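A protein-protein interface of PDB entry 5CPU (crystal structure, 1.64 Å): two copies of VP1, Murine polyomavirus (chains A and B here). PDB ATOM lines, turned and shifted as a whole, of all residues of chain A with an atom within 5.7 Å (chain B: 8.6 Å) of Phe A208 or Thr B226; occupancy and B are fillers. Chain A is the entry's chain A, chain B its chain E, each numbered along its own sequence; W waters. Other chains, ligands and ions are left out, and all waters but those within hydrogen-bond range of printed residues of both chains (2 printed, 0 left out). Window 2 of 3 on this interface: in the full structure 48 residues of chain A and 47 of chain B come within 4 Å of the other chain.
O of Phe A133 sits at hydrogen-bond distance from N of Phe A208, 3.0 Å away.
The guanidinium group of Arg A206 lies within hydrogen-bond range of the backbone carbonyl oxygen of Leu A231.
The backbone carbonyl oxygen (O) of His A131 sits at hydrogen-bond distance from the backbone NH (N) of Asn A210 (2.9 Å).
The side-chain hydroxyl (OG1) of Thr B226 is in hydrogen-bond range of the side-chain hydroxyl (OG1) of Thr B224, 2.7 Å away.
The backbone carbonyl oxygen (O) of Asn B225 is in hydrogen-bond range of the side-chain amino group (NZ) of Lys B94, at 2.8 Å.
1 position is printed for both chains.
Of the 12 pairs that touch across the chains among the printed residues, none has its exchanged pair printed and touching as well.
Of the 12 printed residues of chain A, 6 touch a printed residue of chain B.
Hydrophobic or aromatic side chains of chain A that line the printed part of chain B: Val A132, Tyr A207 and Phe A208.
Hydrophobic or aromatic side chains of chain B that line the printed part of chain A: Phe B223.
OD1 of Asn B225 sits at hydrogen-bond distance from N of Tyr A207 (3.0 Å).
The backbone NH of Gly A209 sits at hydrogen-bond distance from the backbone carbonyl oxygen of Phe B223 (2.8 Å).
The side-chain hydroxyl of Tyr A207 sits at hydrogen-bond distance from the side-chain carboxylate of Glu B96, 2.9 Å away.
The side-chain hydroxyl (OG1) of Thr B224 is in hydrogen-bond range of the backbone carbonyl oxygen (O) of Tyr A207.
Of chain B, only Phe B223, Thr B224 and Thr B226 come within 4 Å of Phe A208.
Thr B226 touches just one residue of chain A: Phe A208.
Gly A209 touches just these residues of chain B: Gln B222 (3.4 Å) and Phe B223 (2.8 Å).
Of the printed residues of chain B, Tyr A207 touches Glu B96 (2.9 Å), Thr B224 (2.6 Å) and Asn B225 (3.0 Å).
Of the printed residues of chain B, Arg A206 touches Asn B225 (3.6 Å).
The nearest residue of chain A that does not touch Thr B226 is Arg A206 (4.04 Å).
The nearest printed residue of chain B that does not touch Val A132 is Thr B224 (7.7 Å).
Water W2 bridges the guanidinium group (NH1) of Arg A206 (2.9 Å) and the side-chain amide nitrogen (ND2) of Asn B225 (3.4 Å).
Water W1 lies within hydrogen-bond range of O of Gly A209 (3.1 Å) and O of Phe B223 (3.4 Å).
Among the printed residues, pairs that only touch across the chains: Val A132 with Phe B223, Arg A206 with Asn B225, Phe A208 with Phe B223, Phe A208 with Thr B224, Phe A208 with Thr B226, Gly A209 with Gln B222, Asn A210 with Leu B221 and Asn A210 with Phe B223.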
ATOM      1  N   HIS A 131       9.915   6.881 -20.094  1.00  0.00           N
ATOM      2  CA  HIS A 131       9.346   6.035 -19.048  1.00  0.00           C
ATOM      3  C   HIS A 131       9.053   6.876 -17.833  1.00  0.00           C
ATOM      4  O   HIS A 131       9.961   7.432 -17.237  1.00  0.00           O
ATOM      5  CB  HIS A 131      10.344   4.926 -18.673  1.00  0.00           C
ATOM      6  CG  HIS A 131      10.598   3.964 -19.787  1.00  0.00           C
ATOM      7  ND1 HIS A 131       9.705   2.971 -20.129  1.00  0.00           N
ATOM      8  CD2 HIS A 131      11.634   3.859 -20.654  1.00  0.00           C
ATOM      9  CE1 HIS A 131      10.184   2.291 -21.157  1.00  0.00           C
ATOM     10  NE2 HIS A 131      11.353   2.809 -21.493  1.00  0.00           N
ATOM     11  N   VAL A 132       7.779   6.954 -17.450  1.00  0.00           N
ATOM     12  CA  VAL A 132       7.403   7.671 -16.242  1.00  0.00           C
ATOM     13  C   VAL A 132       6.356   6.846 -15.517  1.00  0.00           C
ATOM     14  O   VAL A 132       5.478   6.271 -16.146  1.00  0.00           O
ATOM     15  CB  VAL A 132       6.785   9.065 -16.544  1.00  0.00           C
ATOM     16  CG1 VAL A 132       6.698   9.885 -15.258  1.00  0.00           C
ATOM     17  CG2 VAL A 132       7.602   9.814 -17.592  1.00  0.00           C
ATOM     18  N   PHE A 133       6.453   6.777 -14.199  1.00  0.00           N
ATOM     19  CA  PHE A 133       5.337   6.254 -13.418  1.00  0.00           C
ATOM     20  C   PHE A 133       5.104   7.133 -12.214  1.00  0.00           C
ATOM     21  O   PHE A 133       6.011   7.836 -11.761  1.00  0.00           O
ATOM     22  CB  PHE A 133       5.526   4.769 -13.036  1.00  0.00           C
ATOM     23  CG  PHE A 133       6.534   4.520 -11.945  1.00  0.00           C
ATOM     24  CD1 PHE A 133       7.899   4.409 -12.237  1.00  0.00           C
ATOM     25  CD2 PHE A 133       6.118   4.353 -10.621  1.00  0.00           C
ATOM     26  CE1 PHE A 133       8.822   4.156 -11.221  1.00  0.00           C
ATOM     27  CE2 PHE A 133       7.032   4.109  -9.608  1.00  0.00           C
ATOM     28  CZ  PHE A 133       8.390   4.006  -9.906  1.00  0.00           C
ATOM     29  N   ALA A 134       3.880   7.101 -11.702  1.00  0.00           N
ATOM     30  CA  ALA A 134       3.552   7.843 -10.493  1.00  0.00           C
ATOM     31  C   ALA A 134       2.531   7.089  -9.692  1.00  0.00           C
ATOM     32  O   ALA A 134       1.713   6.354 -10.244  1.00  0.00           O
ATOM     33  CB  ALA A 134       3.002   9.228 -10.854  1.00  0.00           C
ATOM     34  N   ARG A 206       4.156  10.657  -5.745  1.00  0.00           N
ATOM     35  CA  ARG A 206       5.570  10.493  -6.093  1.00  0.00           C
ATOM     36  C   ARG A 206       5.656  10.099  -7.550  1.00  0.00           C
ATOM     37  O   ARG A 206       4.935   9.189  -7.996  1.00  0.00           O
ATOM     38  CB  ARG A 206       6.236   9.410  -5.233  1.00  0.00           C
ATOM     39  CG  ARG A 206       5.936   9.475  -3.744  1.00  0.00           C
ATOM     40  CD  ARG A 206       6.427  10.764  -3.085  1.00  0.00           C
ATOM     41  NE  ARG A 206       6.123  10.656  -1.672  1.00  0.00           N
ATOM     42  CZ  ARG A 206       5.221  11.374  -1.009  1.00  0.00           C
ATOM     43  NH1 ARG A 206       4.544  12.360  -1.598  1.00  0.00           N
ATOM     44  NH2 ARG A 206       5.032  11.114   0.271  1.00  0.00           N
ATOM     45  N   TYR A 207       6.523  10.772  -8.310  1.00  0.00           N
ATOM     46  CA  TYR A 207       6.695  10.403  -9.715  1.00  0.00           C
ATOM     47  C   TYR A 207       8.163  10.249 -10.062  1.00  0.00           C
ATOM     48  O   TYR A 207       9.021  10.855  -9.423  1.00  0.00           O
ATOM     49  CB  TYR A 207       6.008  11.391 -10.669  1.00  0.00           C
ATOM     50  CG  TYR A 207       6.540  12.810 -10.625  1.00  0.00           C
ATOM     51  CD1 TYR A 207       7.678  13.184 -11.356  1.00  0.00           C
ATOM     52  CD2 TYR A 207       5.882  13.782  -9.871  1.00  0.00           C
ATOM     53  CE1 TYR A 207       8.155  14.486 -11.309  1.00  0.00           C
ATOM     54  CE2 TYR A 207       6.347  15.090  -9.826  1.00  0.00           C
ATOM     55  CZ  TYR A 207       7.474  15.430 -10.542  1.00  0.00           C
ATOM     56  OH  TYR A 207       7.931  16.717 -10.492  1.00  0.00           O
ATOM     57  N   PHE A 208       8.422   9.405 -11.058  1.00  0.00           N
ATOM     58  CA  PHE A 208       9.784   9.040 -11.448  1.00  0.00           C
ATOM     59  C   PHE A 208       9.817   8.909 -12.957  1.00  0.00           C
ATOM     60  O   PHE A 208       9.080   8.096 -13.534  1.00  0.00           O
ATOM     61  CB  PHE A 208      10.152   7.680 -10.833  1.00  0.00           C
ATOM     62  CG  PHE A 208       9.865   7.573  -9.367  1.00  0.00           C
ATOM     63  CD1 PHE A 208       8.591   7.217  -8.913  1.00  0.00           C
ATOM     64  CD2 PHE A 208      10.869   7.809  -8.434  1.00  0.00           C
ATOM     65  CE1 PHE A 208       8.332   7.115  -7.556  1.00  0.00           C
ATOM     66  CE2 PHE A 208      10.620   7.689  -7.075  1.00  0.00           C
ATOM     67  CZ  PHE A 208       9.346   7.343  -6.637  1.00  0.00           C
ATOM     68  N   GLY A 209      10.680   9.687 -13.610  1.00  0.00           N
ATOM     69  CA  GLY A 209      10.700   9.686 -15.076  1.00  0.00           C
ATOM     70  C   GLY A 209      12.086   9.712 -15.680  1.00  0.00           C
ATOM     71  O   GLY A 209      13.047  10.184 -15.059  1.00  0.00           O
ATOM     72  N   ASN A 210      12.182   9.194 -16.902  1.00  0.00           N
ATOM     73  CA  ASN A 210      13.414   9.333 -17.675  1.00  0.00           C
ATOM     74  C   ASN A 210      13.128   9.401 -19.162  1.00  0.00           C
ATOM     75  O   ASN A 210      12.129   8.861 -19.658  1.00  0.00           O
ATOM     76  CB  ASN A 210      14.434   8.244 -17.336  1.00  0.00           C
ATOM     77  CG  ASN A 210      13.895   6.848 -17.548  1.00  0.00           C
ATOM     78  OD1 ASN A 210      13.677   6.423 -18.677  1.00  0.00           O
ATOM     79  ND2 ASN A 210      13.700   6.119 -16.457  1.00  0.00           N
ATOM     80  N   THR A 229      10.064   0.168  -4.658  1.00  0.00           N
ATOM     81  CA  THR A 229      10.198   1.623  -4.604  1.00  0.00           C
ATOM     82  C   THR A 229       9.490   2.157  -3.360  1.00  0.00           C
ATOM     83  O   THR A 229       8.277   1.985  -3.225  1.00  0.00           O
ATOM     84  CB  THR A 229       9.586   2.273  -5.859  1.00  0.00           C
ATOM     85  OG1 THR A 229      10.198   1.720  -7.033  1.00  0.00           O
ATOM     86  CG2 THR A 229       9.787   3.783  -5.847  1.00  0.00           C
ATOM     87  N   VAL A 230      10.238   2.802  -2.468  1.00  0.00           N
ATOM     88  CA  VAL A 230       9.659   3.354  -1.232  1.00  0.00           C
ATOM     89  C   VAL A 230       8.975   4.675  -1.581  1.00  0.00           C
ATOM     90  O   VAL A 230       9.513   5.461  -2.355  1.00  0.00           O
ATOM     91  CB  VAL A 230      10.721   3.539  -0.119  1.00  0.00           C
ATOM     92  CG1 VAL A 230      10.101   4.138   1.137  1.00  0.00           C
ATOM     93  CG2 VAL A 230      11.363   2.203   0.225  1.00  0.00           C
ATOM     94  N   LEU A 231       7.775   4.894  -1.048  1.00  0.00           N
ATOM     95  CA  LEU A 231       6.970   6.066  -1.412  1.00  0.00           C
ATOM     96  C   LEU A 231       6.878   7.075  -0.265  1.00  0.00           C
ATOM     97  O   LEU A 231       6.285   8.150  -0.414  1.00  0.00           O
ATOM     98  CB  LEU A 231       5.567   5.642  -1.874  1.00  0.00           C
ATOM     99  CG  LEU A 231       5.467   4.796  -3.146  1.00  0.00           C
ATOM    100  CD1 LEU A 231       4.031   4.325  -3.356  1.00  0.00           C
ATOM    101  CD2 LEU A 231       5.951   5.584  -4.360  1.00  0.00           C
ATOM    102  N   VAL B  93      17.976  21.735  -1.714  1.00  0.00           N
ATOM    103  CA  VAL B  93      17.150  22.120  -2.861  1.00  0.00           C
ATOM    104  C   VAL B  93      16.619  20.885  -3.576  1.00  0.00           C
ATOM    105  O   VAL B  93      17.335  19.892  -3.726  1.00  0.00           O
ATOM    106  CB  VAL B  93      17.908  23.072  -3.814  1.00  0.00           C
ATOM    107  CG1 VAL B  93      19.178  22.422  -4.368  1.00  0.00           C
ATOM    108  CG2 VAL B  93      17.005  23.558  -4.951  1.00  0.00           C
ATOM    109  N   LYS B  94      15.344  20.933  -3.955  1.00  0.00           N
ATOM    110  CA  LYS B  94      14.802  19.999  -4.932  1.00  0.00           C
ATOM    111  C   LYS B  94      14.746  20.751  -6.245  1.00  0.00           C
ATOM    112  O   LYS B  94      14.119  21.813  -6.339  1.00  0.00           O
ATOM    113  CB  LYS B  94      13.412  19.492  -4.535  1.00  0.00           C
ATOM    114  CG  LYS B  94      13.434  18.766  -3.201  1.00  0.00           C
ATOM    115  CD  LYS B  94      12.055  18.328  -2.743  1.00  0.00           C
ATOM    116  CE  LYS B  94      11.820  16.865  -3.057  1.00  0.00           C
ATOM    117  NZ  LYS B  94      10.558  16.385  -2.428  1.00  0.00           N
ATOM    118  N   THR B  95      15.424  20.213  -7.249  1.00  0.00           N
ATOM    119  CA  THR B  95      15.469  20.865  -8.557  1.00  0.00           C
ATOM    120  C   THR B  95      15.143  19.876  -9.661  1.00  0.00           C
ATOM    121  O   THR B  95      15.477  18.692  -9.568  1.00  0.00           O
ATOM    122  CB  THR B  95      16.805  21.620  -8.796  1.00  0.00           C
ATOM    123  OG1 THR B  95      16.738  22.361 -10.025  1.00  0.00           O
ATOM    124  CG2 THR B  95      18.003  20.661  -8.865  1.00  0.00           C
ATOM    125  N   GLU B  96      14.469  20.366 -10.695  1.00  0.00           N
ATOM    126  CA  GLU B  96      13.996  19.510 -11.769  1.00  0.00           C
ATOM    127  C   GLU B  96      13.972  20.299 -13.066  1.00  0.00           C
ATOM    128  O   GLU B  96      13.573  21.467 -13.080  1.00  0.00           O
ATOM    129  CB  GLU B  96      12.588  19.011 -11.424  1.00  0.00           C
ATOM    130  CG  GLU B  96      11.999  18.021 -12.421  1.00  0.00           C
ATOM    131  CD  GLU B  96      10.787  17.295 -11.858  1.00  0.00           C
ATOM    132  OE1 GLU B  96      10.761  17.025 -10.652  1.00  0.00           O
ATOM    133  OE2 GLU B  96       9.864  17.004 -12.629  1.00  0.00           O
ATOM    134  N   LEU B 221      17.643  12.668 -19.967  1.00  0.00           N
ATOM    135  CA  LEU B 221      17.215  13.464 -18.806  1.00  0.00           C
ATOM    136  C   LEU B 221      16.417  12.594 -17.860  1.00  0.00           C
ATOM    137  O   LEU B 221      15.642  11.748 -18.296  1.00  0.00           O
ATOM    138  CB  LEU B 221      16.366  14.658 -19.254  1.00  0.00           C
ATOM    139  CG  LEU B 221      16.287  15.815 -18.258  1.00  0.00           C
ATOM    140  CD1 LEU B 221      17.563  16.643 -18.319  1.00  0.00           C
ATOM    141  CD2 LEU B 221      15.086  16.692 -18.571  1.00  0.00           C
ATOM    142  N   GLN B 222      16.639  12.792 -16.564  1.00  0.00           N
ATOM    143  CA  GLN B 222      15.814  12.164 -15.545  1.00  0.00           C
ATOM    144  C   GLN B 222      15.085  13.248 -14.781  1.00  0.00           C
ATOM    145  O   GLN B 222      15.557  14.385 -14.695  1.00  0.00           O
ATOM    146  CB  GLN B 222      16.673  11.362 -14.575  1.00  0.00           C
ATOM    147  CG  GLN B 222      17.255  10.095 -15.170  1.00  0.00           C
ATOM    148  CD  GLN B 222      18.119   9.327 -14.183  1.00  0.00           C
ATOM    149  OE1 GLN B 222      18.436   9.819 -13.094  1.00  0.00           O
ATOM    150  NE2 GLN B 222      18.503   8.113 -14.559  1.00  0.00           N
ATOM    151  N   PHE B 223      13.928  12.893 -14.234  1.00  0.00           N
ATOM    152  CA  PHE B 223      13.151  13.835 -13.431  1.00  0.00           C
ATOM    153  C   PHE B 223      12.340  13.090 -12.394  1.00  0.00           C
ATOM    154  O   PHE B 223      11.781  12.034 -12.681  1.00  0.00           O
ATOM    155  CB  PHE B 223      12.255  14.737 -14.298  1.00  0.00           C
ATOM    156  CG  PHE B 223      11.421  14.006 -15.328  1.00  0.00           C
ATOM    157  CD1 PHE B 223      11.969  13.618 -16.544  1.00  0.00           C
ATOM    158  CD2 PHE B 223      10.065  13.744 -15.093  1.00  0.00           C
ATOM    159  CE1 PHE B 223      11.195  12.959 -17.499  1.00  0.00           C
ATOM    160  CE2 PHE B 223       9.290  13.097 -16.049  1.00  0.00           C
ATOM    161  CZ  PHE B 223       9.856  12.699 -17.252  1.00  0.00           C
ATOM    162  N   THR B 224      12.304  13.625 -11.177  1.00  0.00           N
ATOM    163  CA  THR B 224      11.516  13.031 -10.107  1.00  0.00           C
ATOM    164  C   THR B 224      11.310  14.090  -9.044  1.00  0.00           C
ATOM    165  O   THR B 224      12.160  14.967  -8.885  1.00  0.00           O
ATOM    166  CB  THR B 224      12.208  11.792  -9.464  1.00  0.00           C
ATOM    167  OG1 THR B 224      11.416  11.302  -8.381  1.00  0.00           O
ATOM    168  CG2 THR B 224      13.604  12.131  -8.925  1.00  0.00           C
ATOM    169  N   ASN B 225      10.211  14.000  -8.300  1.00  0.00           N
ATOM    170  CA  ASN B 225      10.016  14.903  -7.168  1.00  0.00           C
ATOM    171  C   ASN B 225      10.505  14.317  -5.832  1.00  0.00           C
ATOM    172  O   ASN B 225      10.134  14.796  -4.751  1.00  0.00           O
ATOM    173  CB  ASN B 225       8.545  15.370  -7.065  1.00  0.00           C
ATOM    174  CG  ASN B 225       7.567  14.237  -6.780  1.00  0.00           C
ATOM    175  OD1 ASN B 225       7.881  13.056  -6.964  1.00  0.00           O
ATOM    176  ND2 ASN B 225       6.367  14.595  -6.312  1.00  0.00           N
ATOM    177  N   THR B 226      11.338  13.277  -5.912  1.00  0.00           N
ATOM    178  CA  THR B 226      11.776  12.551  -4.717  1.00  0.00           C
ATOM    179  C   THR B 226      13.246  12.752  -4.354  1.00  0.00           C
ATOM    180  O   THR B 226      13.713  12.185  -3.346  1.00  0.00           O
ATOM    181  CB  THR B 226      11.538  11.028  -4.868  1.00  0.00           C
ATOM    182  OG1 THR B 226      12.358  10.521  -5.932  1.00  0.00           O
ATOM    183  CG2 THR B 226      10.053  10.721  -5.126  1.00  0.00           C
ATOM    184  N   LEU B 227      13.944  13.574  -5.134  1.00  0.00           N
ATOM    185  CA  LEU B 227      15.388  13.762  -4.988  1.00  0.00           C
ATOM    186  C   LEU B 227      15.722  15.125  -4.386  1.00  0.00           C
ATOM    187  O   LEU B 227      15.360  16.168  -4.945  1.00  0.00           O
ATOM    188  CB  LEU B 227      16.067  13.599  -6.349  1.00  0.00           C
ATOM    189  CG  LEU B 227      17.583  13.778  -6.457  1.00  0.00           C
ATOM    190  CD1 LEU B 227      18.299  12.748  -5.600  1.00  0.00           C
ATOM    191  CD2 LEU B 227      18.025  13.687  -7.912  1.00  0.00           C
ATOM    192  N   THR B 228      16.434  15.097  -3.271  1.00  0.00           N
ATOM    193  CA  THR B 228      16.859  16.298  -2.580  1.00  0.00           C
ATOM    194  C   THR B 228      18.372  16.451  -2.708  1.00  0.00           C
ATOM    195  O   THR B 228      19.115  15.500  -2.472  1.00  0.00           O
ATOM    196  CB  THR B 228      16.463  16.190  -1.104  1.00  0.00           C
ATOM    197  OG1 THR B 228      15.034  16.167  -1.013  1.00  0.00           O
ATOM    198  CG2 THR B 228      17.015  17.348  -0.279  1.00  0.00           C
ATOM    199  N   THR B 229      18.812  17.644  -3.099  1.00  0.00           N
ATOM    200  CA  THR B 229      20.238  17.977  -3.140  1.00  0.00           C
ATOM    201  C   THR B 229      20.602  18.719  -1.859  1.00  0.00           C
ATOM    202  O   THR B 229      20.071  19.795  -1.599  1.00  0.00           O
ATOM    203  CB  THR B 229      20.547  18.853  -4.371  1.00  0.00           C
ATOM    204  OG1 THR B 229      20.167  18.158  -5.568  1.00  0.00           O
ATOM    205  CG2 THR B 229      22.025  19.206  -4.433  1.00  0.00           C
HETATM  206  O   HOH W   1      13.846   9.438 -12.134  1.00  0.00           O
HETATM  207  O   HOH W   2       5.480  14.649  -3.077  1.00  0.00           O
